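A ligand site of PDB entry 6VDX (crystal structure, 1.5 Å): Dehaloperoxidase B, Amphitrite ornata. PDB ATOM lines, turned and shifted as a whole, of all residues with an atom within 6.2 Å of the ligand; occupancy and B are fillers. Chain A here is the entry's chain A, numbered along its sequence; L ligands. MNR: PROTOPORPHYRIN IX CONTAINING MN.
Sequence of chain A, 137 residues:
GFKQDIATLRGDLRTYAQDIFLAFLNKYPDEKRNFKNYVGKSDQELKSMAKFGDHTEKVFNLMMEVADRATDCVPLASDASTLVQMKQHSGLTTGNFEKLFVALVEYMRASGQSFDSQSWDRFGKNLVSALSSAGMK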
ATOM      1  N   PHE A  21     -31.951   2.268  25.201  1.00  0.00           N
ATOM      2  CA  PHE A  21     -30.777   2.058  24.355  1.00  0.00           C
ATOM      3  C   PHE A  21     -30.768   0.603  23.850  1.00  0.00           C
ATOM      4  O   PHE A  21     -30.373   0.332  22.717  1.00  0.00           O
ATOM      5  CB  PHE A  21     -29.513   2.385  25.154  1.00  0.00           C
ATOM      6  CG  PHE A  21     -28.351   2.599  24.227  1.00  0.00           C
ATOM      7  CD1 PHE A  21     -28.277   3.734  23.452  1.00  0.00           C
ATOM      8  CD2 PHE A  21     -27.348   1.650  24.168  1.00  0.00           C
ATOM      9  CE1 PHE A  21     -27.181   3.913  22.620  1.00  0.00           C
ATOM     10  CE2 PHE A  21     -26.306   1.807  23.277  1.00  0.00           C
ATOM     11  CZ  PHE A  21     -26.260   2.915  22.475  1.00  0.00           C
ATOM     12  N   PHE A  24     -33.070   0.270  20.978  1.00  0.00           N
ATOM     13  CA  PHE A  24     -32.341   0.843  19.820  1.00  0.00           C
ATOM     14  C   PHE A  24     -31.377  -0.206  19.229  1.00  0.00           C
ATOM     15  O   PHE A  24     -31.476  -0.479  18.013  1.00  0.00           O
ATOM     16  CB  PHE A  24     -31.664   2.136  20.245  1.00  0.00           C
ATOM     17  CG  PHE A  24     -30.624   2.630  19.299  1.00  0.00           C
ATOM     18  CD1 PHE A  24     -30.982   3.116  18.038  1.00  0.00           C
ATOM     19  CD2 PHE A  24     -29.306   2.716  19.708  1.00  0.00           C
ATOM     20  CE1 PHE A  24     -30.012   3.618  17.169  1.00  0.00           C
ATOM     21  CE2 PHE A  24     -28.352   3.203  18.842  1.00  0.00           C
ATOM     22  CZ  PHE A  24     -28.704   3.677  17.583  1.00  0.00           C
ATOM     23  N   GLU A  31     -26.146  -0.934  14.158  1.00  0.00           N
ATOM     24  CA  GLU A  31     -25.654   0.221  14.947  1.00  0.00           C
ATOM     25  C   GLU A  31     -24.546  -0.231  15.909  1.00  0.00           C
ATOM     26  O   GLU A  31     -23.783   0.628  16.389  1.00  0.00           O
ATOM     27  CB  GLU A  31     -26.819   0.925  15.668  1.00  0.00           C
ATOM     28  CG  GLU A  31     -27.808   1.628  14.724  1.00  0.00           C
ATOM     29  CD  GLU A  31     -27.234   2.892  14.089  1.00  0.00           C
ATOM     30  OE1 GLU A  31     -27.383   3.083  12.884  1.00  0.00           O
ATOM     31  OE2 GLU A  31     -26.561   3.631  14.803  1.00  0.00           O
ATOM     32  N   ASN A  34     -20.903   1.081  15.931  1.00  0.00           N
ATOM     33  CA  ASN A  34     -20.402   2.247  16.677  1.00  0.00           C
ATOM     34  C   ASN A  34     -20.089   1.875  18.128  1.00  0.00           C
ATOM     35  O   ASN A  34     -19.667   2.790  18.879  1.00  0.00           O
ATOM     36  CB  ASN A  34     -21.448   3.370  16.711  1.00  0.00           C
ATOM     37  CG  ASN A  34     -21.886   3.800  15.325  1.00  0.00           C
ATOM     38  OD1 ASN A  34     -21.134   4.467  14.629  1.00  0.00           O
ATOM     39  ND2 ASN A  34     -23.114   3.435  14.943  1.00  0.00           N
ATOM     40  N   PHE A  35     -20.391   0.642  18.535  1.00  0.00           N
ATOM     41  CA  PHE A  35     -20.351   0.146  19.927  1.00  0.00           C
ATOM     42  C   PHE A  35     -19.805  -1.294  19.921  1.00  0.00           C
ATOM     43  O   PHE A  35     -20.478  -2.184  20.439  1.00  0.00           O
ATOM     44  CB  PHE A  35     -21.726   0.184  20.602  1.00  0.00           C
ATOM     45  CG  PHE A  35     -22.415   1.517  20.499  1.00  0.00           C
ATOM     46  CD1 PHE A  35     -22.094   2.543  21.356  1.00  0.00           C
ATOM     47  CD2 PHE A  35     -23.343   1.745  19.507  1.00  0.00           C
ATOM     48  CE1 PHE A  35     -22.711   3.770  21.236  1.00  0.00           C
ATOM     49  CE2 PHE A  35     -23.947   2.977  19.376  1.00  0.00           C
ATOM     50  CZ  PHE A  35     -23.603   4.001  20.214  1.00  0.00           C
ATOM     51  N   TYR A  38     -19.980  -4.098  22.684  1.00  0.00           N
ATOM     52  CA  TYR A  38     -21.325  -4.648  23.035  1.00  0.00           C
ATOM     53  C   TYR A  38     -21.749  -5.825  22.142  1.00  0.00           C
ATOM     54  O   TYR A  38     -22.773  -6.437  22.387  1.00  0.00           O
ATOM     55  CB  TYR A  38     -22.407  -3.550  23.031  1.00  0.00           C
ATOM     56  CG  TYR A  38     -22.123  -2.372  23.939  1.00  0.00           C
ATOM     57  CD1 TYR A  38     -21.408  -2.544  25.104  1.00  0.00           C
ATOM     58  CD2 TYR A  38     -22.638  -1.111  23.674  1.00  0.00           C
ATOM     59  CE1 TYR A  38     -21.099  -1.493  25.956  1.00  0.00           C
ATOM     60  CE2 TYR A  38     -22.344  -0.046  24.512  1.00  0.00           C
ATOM     61  CZ  TYR A  38     -21.574  -0.220  25.660  1.00  0.00           C
ATOM     62  OH  TYR A  38     -21.273   0.818  26.544  1.00  0.00           O
ATOM     63  N   LYS A  51     -19.437   0.270  31.726  1.00  0.00           N
ATOM     64  CA  LYS A  51     -19.472   1.444  30.816  1.00  0.00           C
ATOM     65  C   LYS A  51     -20.804   1.422  30.068  1.00  0.00           C
ATOM     66  O   LYS A  51     -21.227   2.478  29.571  1.00  0.00           O
ATOM     67  CB  LYS A  51     -18.344   1.500  29.785  1.00  0.00           C
ATOM     68  CG  LYS A  51     -16.927   1.523  30.353  1.00  0.00           C
ATOM     69  CD  LYS A  51     -15.852   1.697  29.318  1.00  0.00           C
ATOM     70  CE  LYS A  51     -14.530   1.970  29.997  1.00  0.00           C
ATOM     71  NZ  LYS A  51     -13.525   2.380  28.994  1.00  0.00           N
ATOM     72  N   ASP A  54     -23.066   3.263  32.834  1.00  0.00           N
ATOM     73  CA  ASP A  54     -22.541   4.631  33.054  1.00  0.00           C
ATOM     74  C   ASP A  54     -22.850   5.470  31.809  1.00  0.00           C
ATOM     75  O   ASP A  54     -23.424   6.577  31.958  1.00  0.00           O
ATOM     76  CB  ASP A  54     -21.041   4.569  33.377  1.00  0.00           C
ATOM     77  CG  ASP A  54     -20.403   5.905  33.720  1.00  0.00           C
ATOM     78  OD1 ASP A  54     -20.816   6.474  34.724  1.00  0.00           O
ATOM     79  OD2 ASP A  54     -19.543   6.365  32.936  1.00  0.00           O
ATOM     80  N   HIS A  55     -22.460   4.969  30.649  1.00  0.00           N
ATOM     81  CA  HIS A  55     -22.532   5.680  29.367  1.00  0.00           C
ATOM     82  C   HIS A  55     -24.006   5.942  29.068  1.00  0.00           C
ATOM     83  O   HIS A  55     -24.253   7.027  28.614  1.00  0.00           O
ATOM     84  CB  HIS A  55     -21.820   5.006  28.213  1.00  0.00           C
ATOM     85  CG  HIS A  55     -20.324   5.122  28.370  1.00  0.00           C
ATOM     86  ND1 HIS A  55     -19.491   5.174  27.296  1.00  0.00           N
ATOM     87  CD2 HIS A  55     -19.541   5.268  29.457  1.00  0.00           C
ATOM     88  CE1 HIS A  55     -18.246   5.268  27.721  1.00  0.00           C
ATOM     89  NE2 HIS A  55     -18.240   5.276  29.014  1.00  0.00           N
ATOM     90  N   THR A  56     -24.848   4.927  29.073  1.00  0.00           N
ATOM     91  CA  THR A  56     -26.256   5.107  28.690  1.00  0.00           C
ATOM     92  C   THR A  56     -26.884   6.104  29.643  1.00  0.00           C
ATOM     93  O   THR A  56     -27.612   6.993  29.144  1.00  0.00           O
ATOM     94  CB  THR A  56     -27.096   3.815  28.666  1.00  0.00           C
ATOM     95  OG1 THR A  56     -27.117   3.172  29.951  1.00  0.00           O
ATOM     96  CG2 THR A  56     -26.623   2.856  27.597  1.00  0.00           C
ATOM     97  N   LYS A  58     -25.419   8.654  31.206  1.00  0.00           N
ATOM     98  CA  LYS A  58     -24.865   9.991  30.882  1.00  0.00           C
ATOM     99  C   LYS A  58     -25.473  10.509  29.574  1.00  0.00           C
ATOM    100  O   LYS A  58     -25.768  11.702  29.515  1.00  0.00           O
ATOM    101  CB  LYS A  58     -23.337   9.949  30.826  1.00  0.00           C
ATOM    102  CG  LYS A  58     -22.742   9.841  32.218  1.00  0.00           C
ATOM    103  CD  LYS A  58     -21.250   9.784  32.245  1.00  0.00           C
ATOM    104  CE  LYS A  58     -20.741   9.781  33.685  1.00  0.00           C
ATOM    105  NZ  LYS A  58     -19.314   9.379  33.764  1.00  0.00           N
ATOM    106  N   VAL A  59     -25.622   9.656  28.589  1.00  0.00           N
ATOM    107  CA  VAL A  59     -26.292  10.006  27.300  1.00  0.00           C
ATOM    108  C   VAL A  59     -27.692  10.523  27.628  1.00  0.00           C
ATOM    109  O   VAL A  59     -28.111  11.587  27.119  1.00  0.00           O
ATOM    110  CB  VAL A  59     -26.386   8.787  26.378  1.00  0.00           C
ATOM    111  CG1 VAL A  59     -27.361   8.984  25.237  1.00  0.00           C
ATOM    112  CG2 VAL A  59     -24.989   8.400  25.923  1.00  0.00           C
ATOM    113  N   PHE A  60     -28.417   9.788  28.429  1.00  0.00           N
ATOM    114  CA  PHE A  60     -29.852  10.105  28.713  1.00  0.00           C
ATOM    115  C   PHE A  60     -29.943  11.334  29.604  1.00  0.00           C
ATOM    116  O   PHE A  60     -30.894  12.197  29.406  1.00  0.00           O
ATOM    117  CB  PHE A  60     -30.643   8.914  29.242  1.00  0.00           C
ATOM    118  CG  PHE A  60     -31.222   8.148  28.079  1.00  0.00           C
ATOM    119  CD1 PHE A  60     -30.384   7.371  27.287  1.00  0.00           C
ATOM    120  CD2 PHE A  60     -32.561   8.263  27.723  1.00  0.00           C
ATOM    121  CE1 PHE A  60     -30.866   6.689  26.194  1.00  0.00           C
ATOM    122  CE2 PHE A  60     -33.045   7.568  26.612  1.00  0.00           C
ATOM    123  CZ  PHE A  60     -32.196   6.802  25.848  1.00  0.00           C
ATOM    124  N   LEU A  62     -27.907  13.905  29.486  1.00  0.00           N
ATOM    125  CA  LEU A  62     -27.746  15.057  28.559  1.00  0.00           C
ATOM    126  C   LEU A  62     -28.985  15.191  27.663  1.00  0.00           C
ATOM    127  O   LEU A  62     -29.425  16.347  27.452  1.00  0.00           O
ATOM    128  CB  LEU A  62     -26.459  14.909  27.748  1.00  0.00           C
ATOM    129  CG  LEU A  62     -26.274  15.904  26.597  1.00  0.00           C
ATOM    130  CD1 LEU A  62     -26.266  17.365  27.050  1.00  0.00           C
ATOM    131  CD2 LEU A  62     -24.992  15.625  25.892  1.00  0.00           C
ATOM    132  N   MET A  63     -29.561  14.083  27.208  1.00  0.00           N
ATOM    133  CA  MET A  63     -30.810  14.128  26.400  1.00  0.00           C
ATOM    134  C   MET A  63     -31.877  14.864  27.210  1.00  0.00           C
ATOM    135  O   MET A  63     -32.596  15.656  26.608  1.00  0.00           O
ATOM    136  CB  MET A  63     -31.325  12.741  26.031  1.00  0.00           C
ATOM    137  CG  MET A  63     -32.328  12.786  24.949  1.00  0.00           C
ATOM    138  SD  MET A  63     -33.235  11.287  24.768  1.00  0.00           S
ATOM    139  CE  MET A  63     -32.035  10.217  24.008  1.00  0.00           C
ATOM    140  N   MET A  64     -31.991  14.592  28.500  1.00  0.00           N
ATOM    141  CA  MET A  64     -33.017  15.194  29.369  1.00  0.00           C
ATOM    142  C   MET A  64     -32.709  16.676  29.597  1.00  0.00           C
ATOM    143  O   MET A  64     -33.674  17.457  29.639  1.00  0.00           O
ATOM    144  CB  MET A  64     -33.219  14.508  30.704  1.00  0.00           C
ATOM    145  CG  MET A  64     -33.756  13.107  30.582  1.00  0.00           C
ATOM    146  SD  MET A  64     -35.280  12.840  29.628  1.00  0.00           S
ATOM    147  CE  MET A  64     -34.736  12.434  27.977  1.00  0.00           C
ATOM    148  N   VAL A  66     -31.253  18.667  27.394  1.00  0.00           N
ATOM    149  CA  VAL A  66     -31.543  19.288  26.060  1.00  0.00           C
ATOM    150  C   VAL A  66     -33.068  19.372  25.935  1.00  0.00           C
ATOM    151  O   VAL A  66     -33.574  20.432  25.526  1.00  0.00           O
ATOM    152  CB  VAL A  66     -30.889  18.486  24.918  1.00  0.00           C
ATOM    153  CG1 VAL A  66     -31.310  19.000  23.557  1.00  0.00           C
ATOM    154  CG2 VAL A  66     -29.382  18.523  25.018  1.00  0.00           C
ATOM    155  N   LEU A  83     -23.833  18.551  20.367  1.00  0.00           N
ATOM    156  CA  LEU A  83     -23.965  17.136  19.919  1.00  0.00           C
ATOM    157  C   LEU A  83     -23.194  16.912  18.621  1.00  0.00           C
ATOM    158  O   LEU A  83     -22.685  15.788  18.421  1.00  0.00           O
ATOM    159  CB  LEU A  83     -25.424  16.786  19.738  1.00  0.00           C
ATOM    160  CG  LEU A  83     -26.177  16.618  21.062  1.00  0.00           C
ATOM    161  CD1 LEU A  83     -27.664  16.710  20.815  1.00  0.00           C
ATOM    162  CD2 LEU A  83     -25.775  15.287  21.733  1.00  0.00           C
ATOM    163  N   MET A  86     -19.123  17.092  19.521  1.00  0.00           N
ATOM    164  CA  MET A  86     -18.627  16.054  20.466  1.00  0.00           C
ATOM    165  C   MET A  86     -17.642  15.118  19.762  1.00  0.00           C
ATOM    166  O   MET A  86     -18.036  14.520  18.718  1.00  0.00           O
ATOM    167  CB  MET A  86     -19.776  15.219  21.024  1.00  0.00           C
ATOM    168  CG  MET A  86     -20.267  15.796  22.277  1.00  0.00           C
ATOM    169  SD  MET A  86     -21.835  15.054  22.778  1.00  0.00           S
ATOM    170  CE  MET A  86     -21.210  13.528  23.497  1.00  0.00           C
ATOM    171  N   GLN A  88     -16.970  12.203  20.433  1.00  0.00           N
ATOM    172  CA  GLN A  88     -17.526  10.821  20.439  1.00  0.00           C
ATOM    173  C   GLN A  88     -18.550  10.670  19.301  1.00  0.00           C
ATOM    174  O   GLN A  88     -18.887   9.526  18.966  1.00  0.00           O
ATOM    175  CB  GLN A  88     -18.136  10.467  21.805  1.00  0.00           C
ATOM    176  CG  GLN A  88     -17.110  10.117  22.866  1.00  0.00           C
ATOM    177  CD  GLN A  88     -17.586  10.421  24.264  1.00  0.00           C
ATOM    178  OE1 GLN A  88     -18.154  11.458  24.519  1.00  0.00           O
ATOM    179  NE2 GLN A  88     -17.362   9.482  25.188  1.00  0.00           N
ATOM    180  N   HIS A  89     -19.029  11.792  18.749  1.00  0.00           N
ATOM    181  CA  HIS A  89     -20.019  11.805  17.632  1.00  0.00           C
ATOM    182  C   HIS A  89     -19.328  12.001  16.280  1.00  0.00           C
ATOM    183  O   HIS A  89     -20.078  12.178  15.254  1.00  0.00           O
ATOM    184  CB  HIS A  89     -21.087  12.881  17.908  1.00  0.00           C
ATOM    185  CG  HIS A  89     -21.944  12.552  19.075  1.00  0.00           C
ATOM    186  ND1 HIS A  89     -22.831  13.448  19.638  1.00  0.00           N
ATOM    187  CD2 HIS A  89     -22.081  11.394  19.770  1.00  0.00           C
ATOM    188  CE1 HIS A  89     -23.466  12.876  20.637  1.00  0.00           C
ATOM    189  NE2 HIS A  89     -23.020  11.614  20.746  1.00  0.00           N
ATOM    190  N   LEU A  92     -20.805  10.272  12.765  1.00  0.00           N
ATOM    191  CA  LEU A  92     -22.251   9.916  12.830  1.00  0.00           C
ATOM    192  C   LEU A  92     -23.012  10.762  11.829  1.00  0.00           C
ATOM    193  O   LEU A  92     -22.549  11.873  11.503  1.00  0.00           O
ATOM    194  CB  LEU A  92     -22.818  10.147  14.228  1.00  0.00           C
ATOM    195  CG  LEU A  92     -22.079   9.392  15.333  1.00  0.00           C
ATOM    196  CD1 LEU A  92     -22.804   9.536  16.639  1.00  0.00           C
ATOM    197  CD2 LEU A  92     -21.932   7.926  15.000  1.00  0.00           C
ATOM    198  N   ASN A  96     -28.472   8.110  12.442  1.00  0.00           N
ATOM    199  CA  ASN A  96     -28.161   7.403  13.702  1.00  0.00           C
ATOM    200  C   ASN A  96     -29.078   7.910  14.818  1.00  0.00           C
ATOM    201  O   ASN A  96     -29.610   7.075  15.586  1.00  0.00           O
ATOM    202  CB  ASN A  96     -26.709   7.656  14.115  1.00  0.00           C
ATOM    203  CG  ASN A  96     -25.699   6.968  13.212  1.00  0.00           C
ATOM    204  OD1 ASN A  96     -24.849   7.634  12.592  1.00  0.00           O
ATOM    205  ND2 ASN A  96     -25.789   5.645  13.064  1.00  0.00           N
ATOM    206  N   PHE A  97     -29.289   9.206  14.906  1.00  0.00           N
ATOM    207  CA  PHE A  97     -30.168   9.872  15.901  1.00  0.00           C
ATOM    208  C   PHE A  97     -31.621   9.611  15.571  1.00  0.00           C
ATOM    209  O   PHE A  97     -32.366   9.337  16.487  1.00  0.00           O
ATOM    210  CB  PHE A  97     -29.910  11.364  15.952  1.00  0.00           C
ATOM    211  CG  PHE A  97     -28.591  11.673  16.584  1.00  0.00           C
ATOM    212  CD1 PHE A  97     -27.434  11.590  15.805  1.00  0.00           C
ATOM    213  CD2 PHE A  97     -28.501  12.075  17.897  1.00  0.00           C
ATOM    214  CE1 PHE A  97     -26.192  11.874  16.376  1.00  0.00           C
ATOM    215  CE2 PHE A  97     -27.273  12.373  18.455  1.00  0.00           C
ATOM    216  CZ  PHE A  97     -26.121  12.251  17.693  1.00  0.00           C
ATOM    217  N   GLU A  98     -31.990   9.732  14.298  1.00  0.00           N
ATOM    218  CA  GLU A  98     -33.350   9.361  13.840  1.00  0.00           C
ATOM    219  C   GLU A  98     -33.671   7.960  14.359  1.00  0.00           C
ATOM    220  O   GLU A  98     -34.746   7.796  14.955  1.00  0.00           O
ATOM    221  CB  GLU A  98     -33.411   9.586  12.336  1.00  0.00           C
ATOM    222  CG  GLU A  98     -34.654   9.091  11.673  1.00  0.00           C
ATOM    223  CD  GLU A  98     -34.652   9.436  10.190  1.00  0.00           C
ATOM    224  OE1 GLU A  98     -33.602   9.243   9.540  1.00  0.00           O
ATOM    225  OE2 GLU A  98     -35.685   9.889   9.700  1.00  0.00           O
ATOM    226  N   LEU A 100     -32.304   6.204  16.959  1.00  0.00           N
ATOM    227  CA  LEU A 100     -32.398   6.193  18.424  1.00  0.00           C
ATOM    228  C   LEU A 100     -33.801   6.720  18.801  1.00  0.00           C
ATOM    229  O   LEU A 100     -34.477   6.102  19.634  1.00  0.00           O
ATOM    230  CB  LEU A 100     -31.302   7.070  19.038  1.00  0.00           C
ATOM    231  CG  LEU A 100     -31.424   7.292  20.540  1.00  0.00           C
ATOM    232  CD1 LEU A 100     -31.479   5.997  21.306  1.00  0.00           C
ATOM    233  CD2 LEU A 100     -30.295   8.124  21.093  1.00  0.00           C
ATOM    234  N   PHE A 101     -34.256   7.779  18.129  1.00  0.00           N
ATOM    235  CA  PHE A 101     -35.566   8.407  18.480  1.00  0.00           C
ATOM    236  C   PHE A 101     -36.731   7.569  17.937  1.00  0.00           C
ATOM    237  O   PHE A 101     -37.833   7.682  18.509  1.00  0.00           O
ATOM    238  CB  PHE A 101     -35.596   9.893  18.122  1.00  0.00           C
ATOM    239  CG  PHE A 101     -34.968  10.666  19.245  1.00  0.00           C
ATOM    240  CD1 PHE A 101     -35.731  11.057  20.339  1.00  0.00           C
ATOM    241  CD2 PHE A 101     -33.598  10.923  19.257  1.00  0.00           C
ATOM    242  CE1 PHE A 101     -35.151  11.709  21.412  1.00  0.00           C
ATOM    243  CE2 PHE A 101     -33.039  11.603  20.323  1.00  0.00           C
ATOM    244  CZ  PHE A 101     -33.801  11.991  21.397  1.00  0.00           C
ATOM    245  N   PHE A 123     -39.570  16.041  18.774  1.00  0.00           N
ATOM    246  CA  PHE A 123     -38.291  16.422  19.420  1.00  0.00           C
ATOM    247  C   PHE A 123     -37.101  15.734  18.718  1.00  0.00           C
ATOM    248  O   PHE A 123     -36.169  16.421  18.393  1.00  0.00           O
ATOM    249  CB  PHE A 123     -38.247  16.079  20.894  1.00  0.00           C
ATOM    250  CG  PHE A 123     -36.885  16.330  21.528  1.00  0.00           C
ATOM    251  CD1 PHE A 123     -36.406  17.624  21.729  1.00  0.00           C
ATOM    252  CD2 PHE A 123     -36.213  15.279  22.096  1.00  0.00           C
ATOM    253  CE1 PHE A 123     -35.215  17.827  22.406  1.00  0.00           C
ATOM    254  CE2 PHE A 123     -35.017  15.485  22.742  1.00  0.00           C
ATOM    255  CZ  PHE A 123     -34.528  16.740  22.920  1.00  0.00           C
ATOM    256  N   LEU A 127     -34.478  17.716  16.558  1.00  0.00           N
ATOM    257  CA  LEU A 127     -33.051  17.602  16.980  1.00  0.00           C
ATOM    258  C   LEU A 127     -32.209  17.214  15.767  1.00  0.00           C
ATOM    259  O   LEU A 127     -31.121  17.762  15.598  1.00  0.00           O
ATOM    260  CB  LEU A 127     -32.906  16.599  18.117  1.00  0.00           C
ATOM    261  CG  LEU A 127     -31.470  16.299  18.544  1.00  0.00           C
ATOM    262  CD1 LEU A 127     -30.784  17.513  19.218  1.00  0.00           C
ATOM    263  CD2 LEU A 127     -31.480  15.087  19.449  1.00  0.00           C
HETATM  264  CHA MNR L   1     -21.117   9.151  23.851  1.00  0.00           C
HETATM  265  CHB MNR L   1     -24.949  12.079  24.465  1.00  0.00           C
HETATM  266  CHC MNR L   1     -27.032   9.915  20.507  1.00  0.00           C
HETATM  267  CHD MNR L   1     -22.840   7.461  19.604  1.00  0.00           C
HETATM  268  C1A MNR L   1     -22.046  10.055  24.432  1.00  0.00           C
HETATM  269  C2A MNR L   1     -21.771  10.698  25.727  1.00  0.00           C
HETATM  270  C3A MNR L   1     -22.931  11.541  25.891  1.00  0.00           C
HETATM  271  C4A MNR L   1     -23.716  11.364  24.626  1.00  0.00           C
HETATM  272  CMA MNR L   1     -23.165  12.396  27.062  1.00  0.00           C
HETATM  273  CAA MNR L   1     -20.705  10.514  26.768  1.00  0.00           C
HETATM  274  CBA MNR L   1     -20.877   9.145  27.481  1.00  0.00           C
HETATM  275  CGA MNR L   1     -19.660   8.855  28.366  1.00  0.00           C
HETATM  276  O1A MNR L   1     -18.525   8.983  27.882  1.00  0.00           O
HETATM  277  O2A MNR L   1     -19.809   8.515  29.566  1.00  0.00           O
HETATM  278  C1B MNR L   1     -25.898  11.723  23.431  1.00  0.00           C
HETATM  279  C2B MNR L   1     -27.260  12.387  23.314  1.00  0.00           C
HETATM  280  C3B MNR L   1     -27.838  11.700  22.116  1.00  0.00           C
HETATM  281  C4B MNR L   1     -26.815  10.734  21.633  1.00  0.00           C
HETATM  282  CMB MNR L   1     -27.814  13.454  24.206  1.00  0.00           C
HETATM  283  CAB MNR L   1     -29.144  11.900  21.449  1.00  0.00           C
HETATM  284  CBB MNR L   1     -29.853  12.977  21.761  1.00  0.00           C
HETATM  285  C1C MNR L   1     -26.084   9.037  19.932  1.00  0.00           C
HETATM  286  C2C MNR L   1     -26.427   8.182  18.766  1.00  0.00           C
HETATM  287  C3C MNR L   1     -25.123   7.476  18.511  1.00  0.00           C
HETATM  288  C4C MNR L   1     -24.214   7.936  19.564  1.00  0.00           C
HETATM  289  CMC MNR L   1     -27.648   8.114  17.930  1.00  0.00           C
HETATM  290  CAC MNR L   1     -24.828   6.439  17.551  1.00  0.00           C
HETATM  291  CBC MNR L   1     -25.752   5.599  17.142  1.00  0.00           C
HETATM  292  C1D MNR L   1     -21.985   7.725  20.713  1.00  0.00           C
HETATM  293  C2D MNR L   1     -20.721   6.974  20.862  1.00  0.00           C
HETATM  294  C3D MNR L   1     -20.205   7.483  22.153  1.00  0.00           C
HETATM  295  C4D MNR L   1     -21.227   8.475  22.600  1.00  0.00           C
HETATM  296  CMD MNR L   1     -20.103   5.949  19.914  1.00  0.00           C
HETATM  297  CAD MNR L   1     -18.909   7.087  22.847  1.00  0.00           C
HETATM  298  CBD MNR L   1     -18.885   5.592  23.135  1.00  0.00           C
HETATM  299  CGD MNR L   1     -19.941   5.153  24.120  1.00  0.00           C
HETATM  300  O1D MNR L   1     -20.171   3.913  24.145  1.00  0.00           O
HETATM  301  O2D MNR L   1     -20.520   5.991  24.882  1.00  0.00           O
HETATM  302 MN   MNR L   1     -23.840   9.839  21.957  1.00  0.00          MN
HETATM  303  NA  MNR L   1     -23.149  10.491  23.759  1.00  0.00           N
HETATM  304  NB  MNR L   1     -25.640  10.745  22.417  1.00  0.00           N
HETATM  305  NC  MNR L   1     -24.811   8.886  20.375  1.00  0.00           N
HETATM  306  ND  MNR L   1     -22.250   8.567  21.742  1.00  0.00           N
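A ring nitrogen (NE2) of His 89 binds a manganese atom (MN) of the ligand (2.3 Å). ND1 of His 55 is in hydrogen-bond range of O2D of the ligand, at 2.7 Å. O1A of the ligand lies within hydrogen-bond range of NE2 of Gln 88 (3.0 Å).
A ring nitrogen (ND1) of His 89 lies close to the side-chain sulfur (SD) of Met 86 (3.7 Å). A ring nitrogen (ND1) of His 89 sits at hydrogen-bond distance from the backbone carbonyl oxygen (O) of Leu 83 (2.6 Å). OE2 of Glu 31 lies within hydrogen-bond range of ND2 of Asn 96 (2.8 Å). O of Glu 31 is in hydrogen-bond range of ND2 of Asn 34 (3.2 Å). The side-chain amino group of Lys 58 is in salt-bridge range of the side-chain carboxylate of Asp 54, at 3.1 Å.
Phe 24 touches the ligand (CZ to CBC, 3.6 Å). Glu 31 touches the ligand (OE2 to CBC, 3.2 Å). Asn 34 touches the ligand (O to CMD, 3.4 Å). CZ of Phe 35 touches CHD of the ligand (3.6 Å). Lys 58 touches the ligand (CD to O2A, 3.3 Å). Val 59 touches the ligand. CG of Leu 62 touches CMB of the ligand (3.8 Å). N of Met 63 touches CMB of the ligand (3.5 Å). CD2 of Leu 83 touches C2B of the ligand (3.6 Å). Met 86 touches the ligand (CE to C4A, 3.5 Å). Leu 92 touches the ligand (CD1 to CHD, 3.6 Å). Asn 96 touches the ligand (O to CMC, 3.2 Å). Phe 97 touches the ligand (CE2 to CHC, 3.2 Å). Leu 100 touches the ligand. Phe 101 touches the ligand. Leu 127 touches the ligand. Hydrophobic or aromatic side chains that line the ligand: Phe 24, Phe 35, His 55, Val 59, Leu 62, Leu 83, Met 86, His 89, Leu 92, Phe 97, Leu 100, Phe 101 and Leu 127. 19 residues have an atom within 4 Å of the ligand: Phe 24, Glu 31, Asn 34, Phe 35, His 55, Lys 58, Val 59, Leu 62, Met 63, Leu 83, Met 86, Gln 88, His 89, Leu 92, Asn 96, Phe 97, Leu 100, Phe 101 and Leu 127. The nearest printed residue that does not touch the ligand is Asp 54 (4.01 Å).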
